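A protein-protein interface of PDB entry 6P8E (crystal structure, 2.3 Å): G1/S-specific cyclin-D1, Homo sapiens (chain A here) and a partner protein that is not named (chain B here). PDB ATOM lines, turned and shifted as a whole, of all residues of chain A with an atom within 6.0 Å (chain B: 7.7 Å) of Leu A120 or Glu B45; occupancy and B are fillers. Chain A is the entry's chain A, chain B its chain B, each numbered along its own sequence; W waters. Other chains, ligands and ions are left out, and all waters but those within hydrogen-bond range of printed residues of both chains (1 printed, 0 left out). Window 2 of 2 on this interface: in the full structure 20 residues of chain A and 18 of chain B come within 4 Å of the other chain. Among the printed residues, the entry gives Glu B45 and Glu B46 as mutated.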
ATOM      1  N   PHE A  90     -12.133  19.259 -19.648  1.00  0.00           N
ATOM      2  CA  PHE A  90     -11.119  18.304 -20.080  1.00  0.00           C
ATOM      3  C   PHE A  90     -11.493  17.707 -21.430  1.00  0.00           C
ATOM      4  O   PHE A  90     -10.703  17.733 -22.385  1.00  0.00           O
ATOM      5  CB  PHE A  90     -10.987  17.217 -19.003  1.00  0.00           C
ATOM      6  CG  PHE A  90      -9.791  16.303 -19.160  1.00  0.00           C
ATOM      7  CD1 PHE A  90      -8.530  16.808 -19.439  1.00  0.00           C
ATOM      8  CD2 PHE A  90      -9.936  14.922 -18.983  1.00  0.00           C
ATOM      9  CE1 PHE A  90      -7.428  15.942 -19.562  1.00  0.00           C
ATOM     10  CE2 PHE A  90      -8.850  14.043 -19.099  1.00  0.00           C
ATOM     11  CZ  PHE A  90      -7.592  14.550 -19.395  1.00  0.00           C
ATOM     12  N   LYS A  94     -10.149  18.390 -25.506  1.00  0.00           N
ATOM     13  CA  LYS A  94      -9.694  17.359 -26.426  1.00  0.00           C
ATOM     14  C   LYS A  94     -10.415  17.453 -27.754  1.00  0.00           C
ATOM     15  O   LYS A  94      -9.823  17.198 -28.809  1.00  0.00           O
ATOM     16  CB  LYS A  94      -9.910  15.988 -25.810  1.00  0.00           C
ATOM     17  CG  LYS A  94      -9.003  15.727 -24.618  1.00  0.00           C
ATOM     18  CD  LYS A  94      -9.183  14.307 -24.141  1.00  0.00           C
ATOM     19  CE  LYS A  94      -8.645  14.090 -22.760  1.00  0.00           C
ATOM     20  NZ  LYS A  94      -8.537  12.613 -22.478  1.00  0.00           N
ATOM     21  N   ALA A 103      -4.493  16.983 -17.362  1.00  0.00           N
ATOM     22  CA  ALA A 103      -5.197  16.583 -16.154  1.00  0.00           C
ATOM     23  C   ALA A 103      -4.606  17.250 -14.918  1.00  0.00           C
ATOM     24  O   ALA A 103      -5.341  17.704 -14.038  1.00  0.00           O
ATOM     25  CB  ALA A 103      -5.155  15.066 -16.013  1.00  0.00           C
ATOM     26  N   ARG A 115      -8.448  15.186  -7.739  1.00  0.00           N
ATOM     27  CA  ARG A 115      -7.178  14.550  -8.069  1.00  0.00           C
ATOM     28  C   ARG A 115      -7.199  13.984  -9.479  1.00  0.00           C
ATOM     29  O   ARG A 115      -8.263  13.663 -10.013  1.00  0.00           O
ATOM     30  CB  ARG A 115      -6.863  13.423  -7.086  1.00  0.00           C
ATOM     31  CG  ARG A 115      -6.598  13.895  -5.676  1.00  0.00           C
ATOM     32  CD  ARG A 115      -7.416  13.095  -4.690  1.00  0.00           C
ATOM     33  NE  ARG A 115      -7.191  13.549  -3.324  1.00  0.00           N
ATOM     34  CZ  ARG A 115      -7.262  12.752  -2.268  1.00  0.00           C
ATOM     35  NH1 ARG A 115      -7.560  11.469  -2.438  1.00  0.00           N
ATOM     36  NH2 ARG A 115      -7.042  13.234  -1.056  1.00  0.00           N
ATOM     37  N   PRO A 116      -6.030  13.827 -10.106  1.00  0.00           N
ATOM     38  CA  PRO A 116      -6.015  13.376 -11.506  1.00  0.00           C
ATOM     39  C   PRO A 116      -6.750  12.071 -11.737  1.00  0.00           C
ATOM     40  O   PRO A 116      -7.543  11.983 -12.684  1.00  0.00           O
ATOM     41  CB  PRO A 116      -4.515  13.264 -11.804  1.00  0.00           C
ATOM     42  CG  PRO A 116      -3.917  14.291 -10.946  1.00  0.00           C
ATOM     43  CD  PRO A 116      -4.682  14.206  -9.650  1.00  0.00           C
ATOM     44  N   GLU A 117      -6.521  11.056 -10.892  1.00  0.00           N
ATOM     45  CA  GLU A 117      -7.244   9.792 -11.037  1.00  0.00           C
ATOM     46  C   GLU A 117      -8.756   9.990 -11.015  1.00  0.00           C
ATOM     47  O   GLU A 117      -9.493   9.225 -11.641  1.00  0.00           O
ATOM     48  CB  GLU A 117      -6.824   8.816  -9.933  1.00  0.00           C
ATOM     49  CG  GLU A 117      -5.311   8.787  -9.671  1.00  0.00           C
ATOM     50  CD  GLU A 117      -4.871   9.681  -8.496  1.00  0.00           C
ATOM     51  OE1 GLU A 117      -4.799  10.921  -8.668  1.00  0.00           O
ATOM     52  OE2 GLU A 117      -4.586   9.141  -7.403  1.00  0.00           O
ATOM     53  N   GLU A 118      -9.239  11.001 -10.300  1.00  0.00           N
ATOM     54  CA  GLU A 118     -10.672  11.239 -10.238  1.00  0.00           C
ATOM     55  C   GLU A 118     -11.159  11.905 -11.505  1.00  0.00           C
ATOM     56  O   GLU A 118     -12.286  11.655 -11.951  1.00  0.00           O
ATOM     57  CB  GLU A 118     -11.013  12.098  -9.023  1.00  0.00           C
ATOM     58  CG  GLU A 118     -10.677  11.406  -7.708  1.00  0.00           C
ATOM     59  CD  GLU A 118     -10.638  12.361  -6.512  1.00  0.00           C
ATOM     60  OE1 GLU A 118     -10.329  13.562  -6.692  1.00  0.00           O
ATOM     61  OE2 GLU A 118     -10.919  11.893  -5.384  1.00  0.00           O
ATOM     62  N   LEU A 119     -10.314  12.753 -12.093  1.00  0.00           N
ATOM     63  CA  LEU A 119     -10.673  13.411 -13.342  1.00  0.00           C
ATOM     64  C   LEU A 119     -10.811  12.396 -14.465  1.00  0.00           C
ATOM     65  O   LEU A 119     -11.760  12.458 -15.254  1.00  0.00           O
ATOM     66  CB  LEU A 119      -9.620  14.462 -13.703  1.00  0.00           C
ATOM     67  CG  LEU A 119      -9.915  15.332 -14.925  1.00  0.00           C
ATOM     68  CD1 LEU A 119     -10.929  16.394 -14.561  1.00  0.00           C
ATOM     69  CD2 LEU A 119      -8.640  15.982 -15.433  1.00  0.00           C
ATOM     70  N   LEU A 120      -9.860  11.458 -14.553  1.00  0.00           N
ATOM     71  CA  LEU A 120      -9.901  10.429 -15.584  1.00  0.00           C
ATOM     72  C   LEU A 120     -11.102   9.506 -15.408  1.00  0.00           C
ATOM     73  O   LEU A 120     -11.736   9.116 -16.393  1.00  0.00           O
ATOM     74  CB  LEU A 120      -8.608   9.616 -15.570  1.00  0.00           C
ATOM     75  CG  LEU A 120      -7.313  10.421 -15.679  1.00  0.00           C
ATOM     76  CD1 LEU A 120      -6.103   9.508 -15.817  1.00  0.00           C
ATOM     77  CD2 LEU A 120      -7.407  11.388 -16.823  1.00  0.00           C
ATOM     78  N   GLN A 121     -11.432   9.141 -14.167  1.00  0.00           N
ATOM     79  CA  GLN A 121     -12.584   8.267 -13.970  1.00  0.00           C
ATOM     80  C   GLN A 121     -13.881   9.011 -14.258  1.00  0.00           C
ATOM     81  O   GLN A 121     -14.815   8.448 -14.835  1.00  0.00           O
ATOM     82  CB  GLN A 121     -12.588   7.693 -12.549  1.00  0.00           C
ATOM     83  CG  GLN A 121     -13.560   6.524 -12.367  1.00  0.00           C
ATOM     84  CD  GLN A 121     -13.235   5.309 -13.251  1.00  0.00           C
ATOM     85  OE1 GLN A 121     -12.067   5.008 -13.521  1.00  0.00           O
ATOM     86  NE2 GLN A 121     -14.275   4.602 -13.687  1.00  0.00           N
ATOM     87  N   MET A 122     -13.949  10.282 -13.878  1.00  0.00           N
ATOM     88  CA  MET A 122     -15.116  11.075 -14.223  1.00  0.00           C
ATOM     89  C   MET A 122     -15.231  11.258 -15.725  1.00  0.00           C
ATOM     90  O   MET A 122     -16.343  11.408 -16.244  1.00  0.00           O
ATOM     91  CB  MET A 122     -15.046  12.431 -13.528  1.00  0.00           C
ATOM     92  CG  MET A 122     -16.300  13.283 -13.689  1.00  0.00           C
ATOM     93  SD  MET A 122     -17.741  12.603 -12.818  1.00  0.00           S
ATOM     94  CE  MET A 122     -19.004  13.213 -13.964  1.00  0.00           C
ATOM     95  N   GLU A 123     -14.105  11.268 -16.441  1.00  0.00           N
ATOM     96  CA  GLU A 123     -14.178  11.427 -17.888  1.00  0.00           C
ATOM     97  C   GLU A 123     -14.861  10.226 -18.520  1.00  0.00           C
ATOM     98  O   GLU A 123     -15.655  10.378 -19.450  1.00  0.00           O
ATOM     99  CB  GLU A 123     -12.783  11.633 -18.484  1.00  0.00           C
ATOM    100  CG  GLU A 123     -12.742  11.530 -20.002  1.00  0.00           C
ATOM    101  CD  GLU A 123     -11.327  11.606 -20.589  1.00  0.00           C
ATOM    102  OE1 GLU A 123     -10.435  10.851 -20.144  1.00  0.00           O
ATOM    103  OE2 GLU A 123     -11.107  12.425 -21.506  1.00  0.00           O
ATOM    104  N   LEU A 124     -14.588   9.022 -18.004  1.00  0.00           N
ATOM    105  CA  LEU A 124     -15.251   7.840 -18.541  1.00  0.00           C
ATOM    106  C   LEU A 124     -16.733   7.861 -18.212  1.00  0.00           C
ATOM    107  O   LEU A 124     -17.564   7.458 -19.027  1.00  0.00           O
ATOM    108  CB  LEU A 124     -14.613   6.573 -17.981  1.00  0.00           C
ATOM    109  CG  LEU A 124     -13.128   6.380 -18.244  1.00  0.00           C
ATOM    110  CD1 LEU A 124     -12.659   5.108 -17.562  1.00  0.00           C
ATOM    111  CD2 LEU A 124     -12.908   6.306 -19.735  1.00  0.00           C
ATOM    112  N   LEU A 125     -17.074   8.310 -17.007  1.00  0.00           N
ATOM    113  CA  LEU A 125     -18.473   8.404 -16.631  1.00  0.00           C
ATOM    114  C   LEU A 125     -19.197   9.423 -17.505  1.00  0.00           C
ATOM    115  O   LEU A 125     -20.273   9.135 -18.040  1.00  0.00           O
ATOM    116  CB  LEU A 125     -18.574   8.753 -15.145  1.00  0.00           C
ATOM    117  CG  LEU A 125     -19.969   8.996 -14.573  1.00  0.00           C
ATOM    118  CD1 LEU A 125     -20.874   7.829 -14.919  1.00  0.00           C
ATOM    119  CD2 LEU A 125     -19.920   9.228 -13.055  1.00  0.00           C
ATOM    120  N   PRO B  42      -4.838   2.918 -26.330  1.00  0.00           N
ATOM    121  CA  PRO B  42      -3.765   3.137 -25.349  1.00  0.00           C
ATOM    122  C   PRO B  42      -4.165   4.122 -24.263  1.00  0.00           C
ATOM    123  O   PRO B  42      -4.335   5.317 -24.527  1.00  0.00           O
ATOM    124  CB  PRO B  42      -2.617   3.681 -26.207  1.00  0.00           C
ATOM    125  CG  PRO B  42      -3.304   4.388 -27.343  1.00  0.00           C
ATOM    126  CD  PRO B  42      -4.592   3.635 -27.601  1.00  0.00           C
ATOM    127  N   ASN B  43      -4.322   3.636 -23.037  1.00  0.00           N
ATOM    128  CA  ASN B  43      -4.688   4.500 -21.924  1.00  0.00           C
ATOM    129  C   ASN B  43      -3.423   5.061 -21.286  1.00  0.00           C
ATOM    130  O   ASN B  43      -2.536   4.301 -20.881  1.00  0.00           O
ATOM    131  CB  ASN B  43      -5.519   3.744 -20.893  1.00  0.00           C
ATOM    132  CG  ASN B  43      -5.413   4.350 -19.504  1.00  0.00           C
ATOM    133  OD1 ASN B  43      -6.128   5.299 -19.174  1.00  0.00           O
ATOM    134  ND2 ASN B  43      -4.522   3.797 -18.678  1.00  0.00           N
ATOM    135  N   GLY B  44      -3.344   6.386 -21.199  1.00  0.00           N
ATOM    136  CA  GLY B  44      -2.214   7.023 -20.561  1.00  0.00           C
ATOM    137  C   GLY B  44      -2.634   7.945 -19.435  1.00  0.00           C
ATOM    138  O   GLY B  44      -3.782   7.913 -18.980  1.00  0.00           O
ATOM    139  N   GLU B  45      -1.696   8.774 -18.980  1.00  0.00           N
ATOM    140  CA  GLU B  45      -1.954   9.727 -17.914  1.00  0.00           C
ATOM    141  C   GLU B  45      -2.901  10.854 -18.337  1.00  0.00           C
ATOM    142  O   GLU B  45      -3.415  11.579 -17.476  1.00  0.00           O
ATOM    143  CB  GLU B  45      -0.594  10.241 -17.420  1.00  0.00           C
ATOM    144  CG  GLU B  45      -0.463  11.710 -17.074  1.00  0.00           C
ATOM    145  CD  GLU B  45       0.898  12.015 -16.460  1.00  0.00           C
ATOM    146  OE1 GLU B  45       1.684  12.784 -17.060  1.00  0.00           O
ATOM    147  OE2 GLU B  45       1.190  11.461 -15.379  1.00  0.00           O
ATOM    148  N   GLU B  46      -3.184  11.009 -19.630  1.00  0.00           N
ATOM    149  CA  GLU B  46      -4.179  11.984 -20.058  1.00  0.00           C
ATOM    150  C   GLU B  46      -5.495  11.324 -20.464  1.00  0.00           C
ATOM    151  O   GLU B  46      -6.267  11.908 -21.230  1.00  0.00           O
ATOM    152  CB  GLU B  46      -3.629  12.857 -21.190  1.00  0.00           C
ATOM    153  CG  GLU B  46      -2.388  13.716 -20.792  1.00  0.00           C
ATOM    154  CD  GLU B  46      -2.566  14.542 -19.490  1.00  0.00           C
ATOM    155  OE1 GLU B  46      -1.669  14.518 -18.604  1.00  0.00           O
ATOM    156  OE2 GLU B  46      -3.600  15.225 -19.356  1.00  0.00           O
ATOM    157  N   GLY B  47      -5.757  10.114 -19.968  1.00  0.00           N
ATOM    158  CA  GLY B  47      -7.054   9.483 -20.171  1.00  0.00           C
ATOM    159  C   GLY B  47      -7.289   9.063 -21.607  1.00  0.00           C
ATOM    160  O   GLY B  47      -6.376   8.620 -22.310  1.00  0.00           O
ATOM    161  N   LEU B  48      -8.532   9.213 -22.050  1.00  0.00           N
ATOM    162  CA  LEU B  48      -8.897   8.800 -23.396  1.00  0.00           C
ATOM    163  C   LEU B  48      -8.071   9.554 -24.431  1.00  0.00           C
ATOM    164  O   LEU B  48      -7.921  10.784 -24.329  1.00  0.00           O
ATOM    165  CB  LEU B  48     -10.385   9.034 -23.655  1.00  0.00           C
ATOM    166  CG  LEU B  48     -11.387   8.186 -22.876  1.00  0.00           C
ATOM    167  CD1 LEU B  48     -12.796   8.689 -23.145  1.00  0.00           C
ATOM    168  CD2 LEU B  48     -11.263   6.705 -23.214  1.00  0.00           C
ATOM    169  N   SER B  80     -13.240  -0.503 -19.117  1.00  0.00           N
ATOM    170  CA  SER B  80     -11.890  -0.239 -18.607  1.00  0.00           C
ATOM    171  C   SER B  80     -11.553  -1.177 -17.462  1.00  0.00           C
ATOM    172  O   SER B  80     -11.190  -2.329 -17.690  1.00  0.00           O
ATOM    173  CB  SER B  80     -11.743   1.224 -18.158  1.00  0.00           C
ATOM    174  OG  SER B  80     -12.501   1.502 -16.994  1.00  0.00           O
ATOM    175  N   ILE B  86      -7.957   0.678 -21.468  1.00  0.00           N
ATOM    176  CA  ILE B  86      -9.339   0.925 -21.872  1.00  0.00           C
ATOM    177  C   ILE B  86      -9.621   0.273 -23.215  1.00  0.00           C
ATOM    178  O   ILE B  86      -8.781   0.294 -24.123  1.00  0.00           O
ATOM    179  CB  ILE B  86      -9.657   2.429 -21.932  1.00  0.00           C
ATOM    180  CG1 ILE B  86      -8.943   3.172 -20.799  1.00  0.00           C
ATOM    181  CG2 ILE B  86     -11.159   2.656 -21.860  1.00  0.00           C
ATOM    182  CD1 ILE B  86      -9.060   4.693 -20.889  1.00  0.00           C
HETATM  183  O   HOH W   1      -5.561  12.236 -24.256  1.00  0.00           O
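The side-chain amino group (NZ) of Lys A94 lies within hydrogen-bond range of the backbone carbonyl oxygen (O) of Glu B46 (2.7 Å).
NZ of Lys A94 sits at hydrogen-bond distance from O of Leu B48.
The side-chain carboxylate (OE2) of Glu B46 lies within hydrogen-bond range of the backbone NH (N) of Ala A103 (2.8 Å).
OE1 of Glu A123 sits at hydrogen-bond distance from N of Leu B48 (3.2 Å).
The side-chain amino group of Lys A94 is in salt-bridge range of the side-chain carboxylate of Glu A123.
CZ of Phe A90 touches O of Glu B46, at 3.5 Å.
NZ of Lys A94 touches C of Gly B47, at 3.9 Å.
O of Glu B45 touches CD1 of Leu A120 (3.8 Å).
Leu A120 touches Gly B47.
CA of Gly B47 touches OE1 of Glu A123 (3.6 Å).
Leu B48 touches Leu A124 (CD2 to CD2, 3.9 Å).
Leu A124 touches Ser B80.
Of the printed residues of chain B, Lys A94 touches Glu B46, Gly B47 and Leu B48.
Of chain B, only Glu B45 (3.8 Å) and Gly B47 (3.8 Å) come within 4 Å of Leu A120.
Of the printed residues of chain B, Glu A123 touches Gly B47 and Leu B48.
Of chain A, only Leu A120 (3.8 Å) comes within 4 Å of Glu B45.
Printed residues of chain A within 4 Å of Ser B80: Leu A124 (3.7 Å).
The nearest residue of chain B that does not touch Leu A120 is Glu B46 (4.1 Å).
The nearest residue of chain A that does not touch Glu B45 is Ala A103 (4.2 Å).
The nearest printed residue of chain B that does not touch Lys A94 is Glu B45 (7.2 Å).
Printed residues of chain B that touch a printed residue of chain A: Glu B45, Glu B46, Gly B47, Leu B48 and Ser B80.
Hydrophobic or aromatic side chains of chain B within 4 Å of the printed part of chain A: Leu B48.
Hydrophobic or aromatic side chains of chain A within 4 Å of the printed part of chain B: Phe A90, Ala A103, Leu A120 and Leu A124.
Along chain A the printed residues that touch a printed residue of chain B span positions 90 to 124.
Among the printed residues, 11 pairs touch across the chains.
Among the printed residues, no Asp or Glu carboxylate lies within 4 Å of a Lys or Arg side-chain nitrogen of the other chain.
Water W1 lies within hydrogen-bond range of O of Leu B48 (2.8 Å), O of Glu B46 (3.1 Å) and NZ of Lys A94 (3.5 Å).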
